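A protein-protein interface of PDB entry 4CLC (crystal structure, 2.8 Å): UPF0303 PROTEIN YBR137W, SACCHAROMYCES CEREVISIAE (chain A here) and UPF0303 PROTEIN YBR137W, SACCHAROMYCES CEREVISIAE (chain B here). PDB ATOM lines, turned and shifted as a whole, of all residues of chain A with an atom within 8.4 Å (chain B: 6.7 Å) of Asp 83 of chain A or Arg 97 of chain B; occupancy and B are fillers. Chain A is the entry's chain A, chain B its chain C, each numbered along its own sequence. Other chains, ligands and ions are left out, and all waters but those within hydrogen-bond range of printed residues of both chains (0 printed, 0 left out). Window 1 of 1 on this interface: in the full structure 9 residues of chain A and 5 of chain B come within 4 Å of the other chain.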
ATOM      1  N   ALA A  60      -9.026 -15.429   5.768  1.00  0.00           N
ATOM      2  CA  ALA A  60      -7.991 -15.804   4.804  1.00  0.00           C
ATOM      3  C   ALA A  60      -6.919 -14.716   4.742  1.00  0.00           C
ATOM      4  O   ALA A  60      -7.219 -13.515   4.717  1.00  0.00           O
ATOM      5  CB  ALA A  60      -8.595 -16.065   3.427  1.00  0.00           C
ATOM      6  N   GLY A  79     -15.405 -22.267   7.961  1.00  0.00           N
ATOM      7  CA  GLY A  79     -16.353 -21.242   7.563  1.00  0.00           C
ATOM      8  C   GLY A  79     -15.814 -20.330   6.472  1.00  0.00           C
ATOM      9  O   GLY A  79     -16.456 -19.340   6.108  1.00  0.00           O
ATOM     10  N   SER A  80     -14.623 -20.655   5.967  1.00  0.00           N
ATOM     11  CA  SER A  80     -14.040 -19.950   4.822  1.00  0.00           C
ATOM     12  C   SER A  80     -14.728 -20.394   3.556  1.00  0.00           C
ATOM     13  O   SER A  80     -15.302 -21.483   3.501  1.00  0.00           O
ATOM     14  CB  SER A  80     -12.541 -20.206   4.714  1.00  0.00           C
ATOM     15  OG  SER A  80     -12.284 -21.593   4.851  1.00  0.00           O
ATOM     16  N   ALA A  81     -14.697 -19.541   2.541  1.00  0.00           N
ATOM     17  CA  ALA A  81     -15.347 -19.870   1.292  1.00  0.00           C
ATOM     18  C   ALA A  81     -14.587 -19.228   0.149  1.00  0.00           C
ATOM     19  O   ALA A  81     -13.678 -18.437   0.381  1.00  0.00           O
ATOM     20  CB  ALA A  81     -16.796 -19.413   1.316  1.00  0.00           C
ATOM     21  N   LEU A  82     -14.978 -19.550  -1.081  1.00  0.00           N
ATOM     22  CA  LEU A  82     -14.314 -19.007  -2.252  1.00  0.00           C
ATOM     23  C   LEU A  82     -14.419 -17.477  -2.336  1.00  0.00           C
ATOM     24  O   LEU A  82     -13.570 -16.826  -2.959  1.00  0.00           O
ATOM     25  CB  LEU A  82     -14.889 -19.673  -3.508  1.00  0.00           C
ATOM     26  CG  LEU A  82     -14.373 -19.333  -4.915  1.00  0.00           C
ATOM     27  CD1 LEU A  82     -12.911 -19.643  -5.098  1.00  0.00           C
ATOM     28  CD2 LEU A  82     -15.189 -20.034  -5.949  1.00  0.00           C
ATOM     29  N   ASP A  83     -15.437 -16.910  -1.687  1.00  0.00           N
ATOM     30  CA  ASP A  83     -15.656 -15.477  -1.739  1.00  0.00           C
ATOM     31  C   ASP A  83     -14.536 -14.758  -1.001  1.00  0.00           C
ATOM     32  O   ASP A  83     -14.237 -13.607  -1.284  1.00  0.00           O
ATOM     33  CB  ASP A  83     -17.027 -15.116  -1.169  1.00  0.00           C
ATOM     34  CG  ASP A  83     -17.337 -13.624  -1.272  1.00  0.00           C
ATOM     35  OD1 ASP A  83     -17.504 -13.110  -2.395  1.00  0.00           O
ATOM     36  OD2 ASP A  83     -17.437 -12.957  -0.225  1.00  0.00           O
ATOM     37  N   ASN A  84     -13.904 -15.447  -0.063  1.00  0.00           N
ATOM     38  CA  ASN A  84     -12.699 -14.920   0.561  1.00  0.00           C
ATOM     39  C   ASN A  84     -11.616 -14.678  -0.470  1.00  0.00           C
ATOM     40  O   ASN A  84     -10.949 -13.651  -0.444  1.00  0.00           O
ATOM     41  CB  ASN A  84     -12.175 -15.874   1.633  1.00  0.00           C
ATOM     42  CG  ASN A  84     -13.002 -15.840   2.898  1.00  0.00           C
ATOM     43  OD1 ASN A  84     -13.628 -16.835   3.275  1.00  0.00           O
ATOM     44  ND2 ASN A  84     -12.998 -14.693   3.572  1.00  0.00           N
ATOM     45  N   ASP A  85     -11.453 -15.639  -1.376  1.00  0.00           N
ATOM     46  CA  ASP A  85     -10.472 -15.554  -2.448  1.00  0.00           C
ATOM     47  C   ASP A  85     -10.777 -14.377  -3.364  1.00  0.00           C
ATOM     48  O   ASP A  85      -9.893 -13.611  -3.753  1.00  0.00           O
ATOM     49  CB  ASP A  85     -10.439 -16.859  -3.236  1.00  0.00           C
ATOM     50  CG  ASP A  85      -9.876 -18.010  -2.425  1.00  0.00           C
ATOM     51  OD1 ASP A  85      -9.758 -17.842  -1.198  1.00  0.00           O
ATOM     52  OD2 ASP A  85      -9.546 -19.071  -3.009  1.00  0.00           O
ATOM     53  N   PHE A  86     -12.042 -14.211  -3.692  1.00  0.00           N
ATOM     54  CA  PHE A  86     -12.417 -13.058  -4.482  1.00  0.00           C
ATOM     55  C   PHE A  86     -12.079 -11.734  -3.774  1.00  0.00           C
ATOM     56  O   PHE A  86     -11.666 -10.768  -4.412  1.00  0.00           O
ATOM     57  CB  PHE A  86     -13.899 -13.132  -4.822  1.00  0.00           C
ATOM     58  CG  PHE A  86     -14.200 -14.031  -5.989  1.00  0.00           C
ATOM     59  CD1 PHE A  86     -14.040 -13.571  -7.298  1.00  0.00           C
ATOM     60  CD2 PHE A  86     -14.636 -15.333  -5.784  1.00  0.00           C
ATOM     61  CE1 PHE A  86     -14.321 -14.369  -8.366  1.00  0.00           C
ATOM     62  CE2 PHE A  86     -14.916 -16.146  -6.858  1.00  0.00           C
ATOM     63  CZ  PHE A  86     -14.758 -15.652  -8.154  1.00  0.00           C
ATOM     64  N   TRP A  87     -12.242 -11.690  -2.455  1.00  0.00           N
ATOM     65  CA  TRP A  87     -11.948 -10.469  -1.724  1.00  0.00           C
ATOM     66  C   TRP A  87     -10.443 -10.229  -1.707  1.00  0.00           C
ATOM     67  O   TRP A  87      -9.985  -9.114  -1.956  1.00  0.00           O
ATOM     68  CB  TRP A  87     -12.522 -10.522  -0.303  1.00  0.00           C
ATOM     69  CG  TRP A  87     -13.968 -10.133  -0.263  1.00  0.00           C
ATOM     70  CD1 TRP A  87     -15.034 -10.967  -0.133  1.00  0.00           C
ATOM     71  CD2 TRP A  87     -14.508  -8.806  -0.367  1.00  0.00           C
ATOM     72  NE1 TRP A  87     -16.206 -10.250  -0.152  1.00  0.00           N
ATOM     73  CE2 TRP A  87     -15.911  -8.922  -0.294  1.00  0.00           C
ATOM     74  CE3 TRP A  87     -13.941  -7.536  -0.501  1.00  0.00           C
ATOM     75  CZ2 TRP A  87     -16.759  -7.814  -0.361  1.00  0.00           C
ATOM     76  CZ3 TRP A  87     -14.785  -6.437  -0.567  1.00  0.00           C
ATOM     77  CH2 TRP A  87     -16.183  -6.585  -0.502  1.00  0.00           C
ATOM     78  N   ILE A  88      -9.676 -11.281  -1.440  1.00  0.00           N
ATOM     79  CA  ILE A  88      -8.232 -11.176  -1.500  1.00  0.00           C
ATOM     80  C   ILE A  88      -7.767 -10.600  -2.852  1.00  0.00           C
ATOM     81  O   ILE A  88      -6.854  -9.790  -2.901  1.00  0.00           O
ATOM     82  CB  ILE A  88      -7.569 -12.536  -1.276  1.00  0.00           C
ATOM     83  CG1 ILE A  88      -7.857 -13.035   0.141  1.00  0.00           C
ATOM     84  CG2 ILE A  88      -6.072 -12.444  -1.553  1.00  0.00           C
ATOM     85  CD1 ILE A  88      -7.036 -14.254   0.573  1.00  0.00           C
ATOM     86  N   GLN A  89      -8.410 -11.014  -3.942  1.00  0.00           N
ATOM     87  CA  GLN A  89      -8.024 -10.562  -5.272  1.00  0.00           C
ATOM     88  C   GLN A  89      -8.384  -9.108  -5.469  1.00  0.00           C
ATOM     89  O   GLN A  89      -7.560  -8.307  -5.907  1.00  0.00           O
ATOM     90  CB  GLN A  89      -8.692 -11.414  -6.358  1.00  0.00           C
ATOM     91  CG  GLN A  89      -8.128 -12.807  -6.455  1.00  0.00           C
ATOM     92  CD  GLN A  89      -6.657 -12.818  -6.856  1.00  0.00           C
ATOM     93  OE1 GLN A  89      -6.306 -12.468  -7.990  1.00  0.00           O
ATOM     94  NE2 GLN A  89      -5.790 -13.215  -5.926  1.00  0.00           N
ATOM     95  N   ARG A  90      -9.629  -8.792  -5.126  1.00  0.00           N
ATOM     96  CA  ARG A  90     -10.211  -7.488  -5.372  1.00  0.00           C
ATOM     97  C   ARG A  90      -9.644  -6.393  -4.494  1.00  0.00           C
ATOM     98  O   ARG A  90      -9.574  -5.241  -4.925  1.00  0.00           O
ATOM     99  CB  ARG A  90     -11.711  -7.552  -5.170  1.00  0.00           C
ATOM    100  CG  ARG A  90     -12.397  -8.419  -6.152  1.00  0.00           C
ATOM    101  CD  ARG A  90     -13.860  -8.388  -5.945  1.00  0.00           C
ATOM    102  NE  ARG A  90     -14.344  -7.026  -5.766  1.00  0.00           N
ATOM    103  CZ  ARG A  90     -14.856  -6.563  -4.629  1.00  0.00           C
ATOM    104  NH1 ARG A  90     -14.951  -7.363  -3.577  1.00  0.00           N
ATOM    105  NH2 ARG A  90     -15.275  -5.306  -4.546  1.00  0.00           N
ATOM    106  N   LYS A 123     -16.539  -4.890  -9.393  1.00  0.00           N
ATOM    107  CA  LYS A 123     -16.356  -6.335  -9.386  1.00  0.00           C
ATOM    108  C   LYS A 123     -14.880  -6.737  -9.327  1.00  0.00           C
ATOM    109  O   LYS A 123     -14.553  -7.791  -8.796  1.00  0.00           O
ATOM    110  CB  LYS A 123     -17.029  -6.961 -10.616  1.00  0.00           C
ATOM    111  CG  LYS A 123     -18.480  -7.392 -10.363  1.00  0.00           C
ATOM    112  CD  LYS A 123     -19.364  -7.315 -11.605  1.00  0.00           C
ATOM    113  CE  LYS A 123     -19.830  -5.887 -11.883  1.00  0.00           C
ATOM    114  NZ  LYS A 123     -20.998  -5.843 -12.817  1.00  0.00           N
ATOM    115  N   SER A 149      -8.859 -10.966   5.018  1.00  0.00           N
ATOM    116  CA  SER A 149     -10.288 -10.897   4.731  1.00  0.00           C
ATOM    117  C   SER A 149     -11.096 -11.808   5.639  1.00  0.00           C
ATOM    118  O   SER A 149     -10.660 -12.915   5.937  1.00  0.00           O
ATOM    119  CB  SER A 149     -10.560 -11.268   3.273  1.00  0.00           C
ATOM    120  OG  SER A 149     -11.948 -11.429   3.038  1.00  0.00           O
ATOM    121  N   GLY A 150     -12.304 -11.360   5.990  1.00  0.00           N
ATOM    122  CA  GLY A 150     -13.223 -12.084   6.862  1.00  0.00           C
ATOM    123  C   GLY A 150     -13.515 -11.459   8.223  1.00  0.00           C
ATOM    124  O   GLY A 150     -14.401 -11.922   8.950  1.00  0.00           O
ATOM    125  N   LYS B  92     -26.917 -22.327  -7.258  1.00  0.00           N
ATOM    126  CA  LYS B  92     -25.847 -23.250  -6.887  1.00  0.00           C
ATOM    127  C   LYS B  92     -24.514 -22.524  -6.801  1.00  0.00           C
ATOM    128  O   LYS B  92     -23.706 -22.779  -5.906  1.00  0.00           O
ATOM    129  CB  LYS B  92     -25.783 -24.402  -7.890  1.00  0.00           C
ATOM    130  CG  LYS B  92     -24.783 -25.486  -7.594  1.00  0.00           C
ATOM    131  CD  LYS B  92     -24.984 -26.711  -8.522  1.00  0.00           C
ATOM    132  CE  LYS B  92     -24.717 -26.399 -10.010  1.00  0.00           C
ATOM    133  NZ  LYS B  92     -23.303 -25.966 -10.245  1.00  0.00           N
ATOM    134  N   LYS B  93     -24.304 -21.603  -7.726  1.00  0.00           N
ATOM    135  CA  LYS B  93     -23.079 -20.862  -7.766  1.00  0.00           C
ATOM    136  C   LYS B  93     -22.925 -20.017  -6.488  1.00  0.00           C
ATOM    137  O   LYS B  93     -21.856 -20.015  -5.863  1.00  0.00           O
ATOM    138  CB  LYS B  93     -23.046 -20.011  -9.038  1.00  0.00           C
ATOM    139  CG  LYS B  93     -21.711 -19.341  -9.282  1.00  0.00           C
ATOM    140  CD  LYS B  93     -21.495 -19.013 -10.731  1.00  0.00           C
ATOM    141  CE  LYS B  93     -20.006 -18.932 -11.020  1.00  0.00           C
ATOM    142  NZ  LYS B  93     -19.753 -18.741 -12.476  1.00  0.00           N
ATOM    143  N   THR B  94     -23.997 -19.322  -6.095  1.00  0.00           N
ATOM    144  CA  THR B  94     -24.044 -18.588  -4.824  1.00  0.00           C
ATOM    145  C   THR B  94     -23.703 -19.474  -3.616  1.00  0.00           C
ATOM    146  O   THR B  94     -22.791 -19.182  -2.849  1.00  0.00           O
ATOM    147  CB  THR B  94     -25.458 -17.978  -4.563  1.00  0.00           C
ATOM    148  OG1 THR B  94     -25.774 -16.968  -5.527  1.00  0.00           O
ATOM    149  CG2 THR B  94     -25.545 -17.389  -3.150  1.00  0.00           C
ATOM    150  N   ALA B  95     -24.458 -20.553  -3.443  1.00  0.00           N
ATOM    151  CA  ALA B  95     -24.255 -21.452  -2.314  1.00  0.00           C
ATOM    152  C   ALA B  95     -22.822 -21.956  -2.238  1.00  0.00           C
ATOM    153  O   ALA B  95     -22.233 -21.990  -1.162  1.00  0.00           O
ATOM    154  CB  ALA B  95     -25.220 -22.629  -2.399  1.00  0.00           C
ATOM    155  N   LEU B  96     -22.263 -22.353  -3.376  1.00  0.00           N
ATOM    156  CA  LEU B  96     -20.938 -22.951  -3.377  1.00  0.00           C
ATOM    157  C   LEU B  96     -19.897 -21.895  -3.093  1.00  0.00           C
ATOM    158  O   LEU B  96     -18.931 -22.149  -2.378  1.00  0.00           O
ATOM    159  CB  LEU B  96     -20.652 -23.669  -4.708  1.00  0.00           C
ATOM    160  CG  LEU B  96     -21.185 -25.106  -4.829  1.00  0.00           C
ATOM    161  CD1 LEU B  96     -21.091 -25.639  -6.228  1.00  0.00           C
ATOM    162  CD2 LEU B  96     -20.435 -26.002  -3.884  1.00  0.00           C
ATOM    163  N   ARG B  97     -20.115 -20.703  -3.629  1.00  0.00           N
ATOM    164  CA  ARG B  97     -19.173 -19.603  -3.448  1.00  0.00           C
ATOM    165  C   ARG B  97     -19.127 -19.033  -2.022  1.00  0.00           C
ATOM    166  O   ARG B  97     -18.042 -18.783  -1.480  1.00  0.00           O
ATOM    167  CB  ARG B  97     -19.490 -18.459  -4.419  1.00  0.00           C
ATOM    168  CG  ARG B  97     -18.600 -17.244  -4.200  1.00  0.00           C
ATOM    169  CD  ARG B  97     -18.854 -16.197  -5.229  1.00  0.00           C
ATOM    170  NE  ARG B  97     -18.223 -14.935  -4.866  1.00  0.00           N
ATOM    171  CZ  ARG B  97     -17.749 -14.059  -5.742  1.00  0.00           C
ATOM    172  NH1 ARG B  97     -17.812 -14.314  -7.044  1.00  0.00           N
ATOM    173  NH2 ARG B  97     -17.206 -12.939  -5.312  1.00  0.00           N
ATOM    174  N   PHE B  98     -20.294 -18.789  -1.435  1.00  0.00           N
ATOM    175  CA  PHE B  98     -20.334 -18.129  -0.147  1.00  0.00           C
ATOM    176  C   PHE B  98     -20.371 -19.063   1.074  1.00  0.00           C
ATOM    177  O   PHE B  98     -20.138 -18.617   2.202  1.00  0.00           O
ATOM    178  CB  PHE B  98     -21.536 -17.191  -0.109  1.00  0.00           C
ATOM    179  CG  PHE B  98     -21.457 -16.054  -1.090  1.00  0.00           C
ATOM    180  CD1 PHE B  98     -20.724 -14.914  -0.787  1.00  0.00           C
ATOM    181  CD2 PHE B  98     -22.123 -16.124  -2.315  1.00  0.00           C
ATOM    182  CE1 PHE B  98     -20.643 -13.874  -1.687  1.00  0.00           C
ATOM    183  CE2 PHE B  98     -22.046 -15.085  -3.221  1.00  0.00           C
ATOM    184  CZ  PHE B  98     -21.308 -13.952  -2.903  1.00  0.00           C
ATOM    185  N   GLY B  99     -20.618 -20.350   0.866  1.00  0.00           N
ATOM    186  CA  GLY B  99     -20.718 -21.267   1.985  1.00  0.00           C
ATOM    187  C   GLY B  99     -21.972 -21.162   2.857  1.00  0.00           C
ATOM    188  O   GLY B  99     -21.956 -21.541   4.035  1.00  0.00           O
ATOM    189  N   HIS B 100     -23.066 -20.656   2.299  1.00  0.00           N
ATOM    190  CA  HIS B 100     -24.353 -20.730   2.983  1.00  0.00           C
ATOM    191  C   HIS B 100     -25.430 -21.027   1.954  1.00  0.00           C
ATOM    192  O   HIS B 100     -25.156 -20.979   0.765  1.00  0.00           O
ATOM    193  CB  HIS B 100     -24.654 -19.439   3.746  1.00  0.00           C
ATOM    194  CG  HIS B 100     -23.712 -19.175   4.878  1.00  0.00           C
ATOM    195  ND1 HIS B 100     -22.694 -18.249   4.805  1.00  0.00           N
ATOM    196  CD2 HIS B 100     -23.623 -19.734   6.109  1.00  0.00           C
ATOM    197  CE1 HIS B 100     -22.016 -18.246   5.938  1.00  0.00           C
ATOM    198  NE2 HIS B 100     -22.558 -19.140   6.746  1.00  0.00           N
ATOM    199  N   PHE B 118     -22.526  -7.777  -2.722  1.00  0.00           N
ATOM    200  CA  PHE B 118     -21.448  -8.755  -2.845  1.00  0.00           C
ATOM    201  C   PHE B 118     -20.535  -8.637  -4.067  1.00  0.00           C
ATOM    202  O   PHE B 118     -19.682  -9.495  -4.264  1.00  0.00           O
ATOM    203  CB  PHE B 118     -22.054 -10.150  -2.797  1.00  0.00           C
ATOM    204  CG  PHE B 118     -22.949 -10.360  -1.627  1.00  0.00           C
ATOM    205  CD1 PHE B 118     -22.408 -10.575  -0.362  1.00  0.00           C
ATOM    206  CD2 PHE B 118     -24.328 -10.321  -1.786  1.00  0.00           C
ATOM    207  CE1 PHE B 118     -23.232 -10.768   0.724  1.00  0.00           C
ATOM    208  CE2 PHE B 118     -25.166 -10.511  -0.711  1.00  0.00           C
ATOM    209  CZ  PHE B 118     -24.620 -10.733   0.550  1.00  0.00           C
ATOM    210  N   PHE B 119     -20.757  -7.624  -4.899  1.00  0.00           N
ATOM    211  CA  PHE B 119     -19.917  -7.349  -6.071  1.00  0.00           C
ATOM    212  C   PHE B 119     -19.823  -8.540  -7.013  1.00  0.00           C
ATOM    213  O   PHE B 119     -18.745  -9.025  -7.336  1.00  0.00           O
ATOM    214  CB  PHE B 119     -18.540  -6.891  -5.609  1.00  0.00           C
ATOM    215  CG  PHE B 119     -18.615  -5.759  -4.631  1.00  0.00           C
ATOM    216  CD1 PHE B 119     -18.747  -4.451  -5.078  1.00  0.00           C
ATOM    217  CD2 PHE B 119     -18.608  -5.999  -3.261  1.00  0.00           C
ATOM    218  CE1 PHE B 119     -18.842  -3.406  -4.188  1.00  0.00           C
ATOM    219  CE2 PHE B 119     -18.703  -4.948  -2.366  1.00  0.00           C
ATOM    220  CZ  PHE B 119     -18.824  -3.650  -2.838  1.00  0.00           C
ATOM    221  N   VAL B 120     -20.987  -9.024  -7.416  1.00  0.00           N
ATOM    222  CA  VAL B 120     -21.101 -10.165  -8.294  1.00  0.00           C
ATOM    223  C   VAL B 120     -22.190  -9.813  -9.288  1.00  0.00           C
ATOM    224  O   VAL B 120     -23.067  -9.005  -8.978  1.00  0.00           O
ATOM    225  CB  VAL B 120     -21.469 -11.460  -7.532  1.00  0.00           C
ATOM    226  CG1 VAL B 120     -20.530 -11.689  -6.383  1.00  0.00           C
ATOM    227  CG2 VAL B 120     -22.883 -11.389  -7.015  1.00  0.00           C
ATOM    228  N   GLU B 124     -25.359 -13.989 -13.025  1.00  0.00           N
ATOM    229  CA  GLU B 124     -24.590 -15.178 -12.734  1.00  0.00           C
ATOM    230  C   GLU B 124     -24.945 -15.849 -11.399  1.00  0.00           C
ATOM    231  O   GLU B 124     -24.627 -17.022 -11.195  1.00  0.00           O
ATOM    232  CB  GLU B 124     -23.095 -14.824 -12.771  1.00  0.00           C
ATOM    233  CG  GLU B 124     -22.132 -16.014 -12.735  1.00  0.00           C
ATOM    234  CD  GLU B 124     -20.694 -15.607 -12.984  1.00  0.00           C
ATOM    235  OE1 GLU B 124     -20.414 -14.383 -12.960  1.00  0.00           O
ATOM    236  OE2 GLU B 124     -19.852 -16.507 -13.222  1.00  0.00           O
ATOM    237  N   TYR B 125     -25.653 -15.151 -10.512  1.00  0.00           N
ATOM    238  CA  TYR B 125     -25.615 -15.531  -9.092  1.00  0.00           C
ATOM    239  C   TYR B 125     -26.894 -15.888  -8.326  1.00  0.00           C
ATOM    240  O   TYR B 125     -26.810 -16.763  -7.486  1.00  0.00           O
ATOM    241  CB  TYR B 125     -24.824 -14.521  -8.328  1.00  0.00           C
ATOM    242  CG  TYR B 125     -23.375 -14.954  -8.358  1.00  0.00           C
ATOM    243  CD1 TYR B 125     -22.916 -15.968  -7.524  1.00  0.00           C
ATOM    244  CD2 TYR B 125     -22.474 -14.391  -9.261  1.00  0.00           C
ATOM    245  CE1 TYR B 125     -21.584 -16.373  -7.555  1.00  0.00           C
ATOM    246  CE2 TYR B 125     -21.153 -14.795  -9.300  1.00  0.00           C
ATOM    247  CZ  TYR B 125     -20.710 -15.783  -8.448  1.00  0.00           C
ATOM    248  OH  TYR B 125     -19.390 -16.168  -8.493  1.00  0.00           O
ATOM    249  N   LEU B 133     -26.192 -26.470   0.695  1.00  0.00           N
ATOM    250  CA  LEU B 133     -25.007 -27.311   0.630  1.00  0.00           C
ATOM    251  C   LEU B 133     -25.230 -28.655   1.324  1.00  0.00           C
ATOM    252  O   LEU B 133     -25.944 -28.729   2.317  1.00  0.00           O
ATOM    253  CB  LEU B 133     -23.811 -26.584   1.250  1.00  0.00           C
ATOM    254  CG  LEU B 133     -23.410 -25.280   0.548  1.00  0.00           C
ATOM    255  CD1 LEU B 133     -22.273 -24.554   1.254  1.00  0.00           C
ATOM    256  CD2 LEU B 133     -23.052 -25.569  -0.907  1.00  0.00           C
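N of Leu 82 of chain A sits at hydrogen-bond distance from O of Arg 97 of chain B, at 3.2 Å.
The side-chain carboxylate (OD1) of Asp 83 of chain A is in salt-bridge range of the guanidinium group (NH2) of Arg 97 of chain B (2.9 Å).
Among the printed residues, merely in contact across the chains: Ala 81 of chain A with Arg 97 of chain B (3.1 Å), Phe 86 of chain A with Arg 97 of chain B (3.3 Å), Asp 83 of chain A with Phe 98 of chain B (3.3 Å), Arg 90 of chain A with Phe 119 of chain B (3.4 Å), Lys 123 of chain A with Phe 119 of chain B (3.4 Å), Trp 87 of chain A with Phe 119 of chain B (3.5 Å), Ala 81 of chain A with Phe 98 of chain B (3.5 Å) and Ala 81 of chain A with Gly 99 of chain B (3.96 Å).
Hydrophobic or aromatic side chains of chain B that line the printed part of chain A: Phe 98 and Phe 119.
Of the 16 printed residues of chain A, 7 touch a printed residue of chain B.
Among the printed residues, Asp or Glu carboxylates within 4 Å of a Lys or Arg side-chain nitrogen of the other chain: Asp 83 of chain A with Arg 97 of chain B.
Printed residues of chain B within 4 Å of Asp 83 of chain A: Arg 97 (2.9 Å) and Phe 98 (3.3 Å).
Of the printed residues of chain A, Arg 97 of chain B touches Ala 81 (3.1 Å), Leu 82 (3.2 Å), Asp 83 (2.9 Å) and Phe 86 (3.3 Å).
Of the printed residues of chain B, Leu 82 of chain A touches Arg 97.
Printed residues of chain B within 4 Å of Phe 86 of chain A: Arg 97 (3.3 Å).
Printed residues of chain B within 4 Å of Ala 81 of chain A: Arg 97 (3.1 Å), Phe 98 (3.5 Å) and Gly 99 (3.96 Å).
The nearest residue of chain B that does not touch Asp 83 of chain A is Phe 118 of chain B (4.6 Å).
The nearest residue of chain A that does not touch Arg 97 of chain B is Asn 84 of chain A (5.5 Å).
The nearest printed residue of chain A that does not touch Phe 119 of chain B is Asp 83 of chain A (6.5 Å).
The backbone NH of Ala 81 of chain A lies within hydrogen-bond range of the side-chain amide oxygen of Asn 84 of chain A (3.0 Å).
OD2 of Asp 83 of chain A sits at hydrogen-bond distance from NE1 of Trp 87 of chain A, 3.0 Å away.
The guanidinium group of Arg 90 of chain A lies close to the backbone carbonyl oxygen of Lys 123 of chain A, at 3.1 Å.
The guanidinium group of Arg 97 of chain B is in hydrogen-bond range of the side-chain hydroxyl of Tyr 125 of chain B (2.8 Å).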
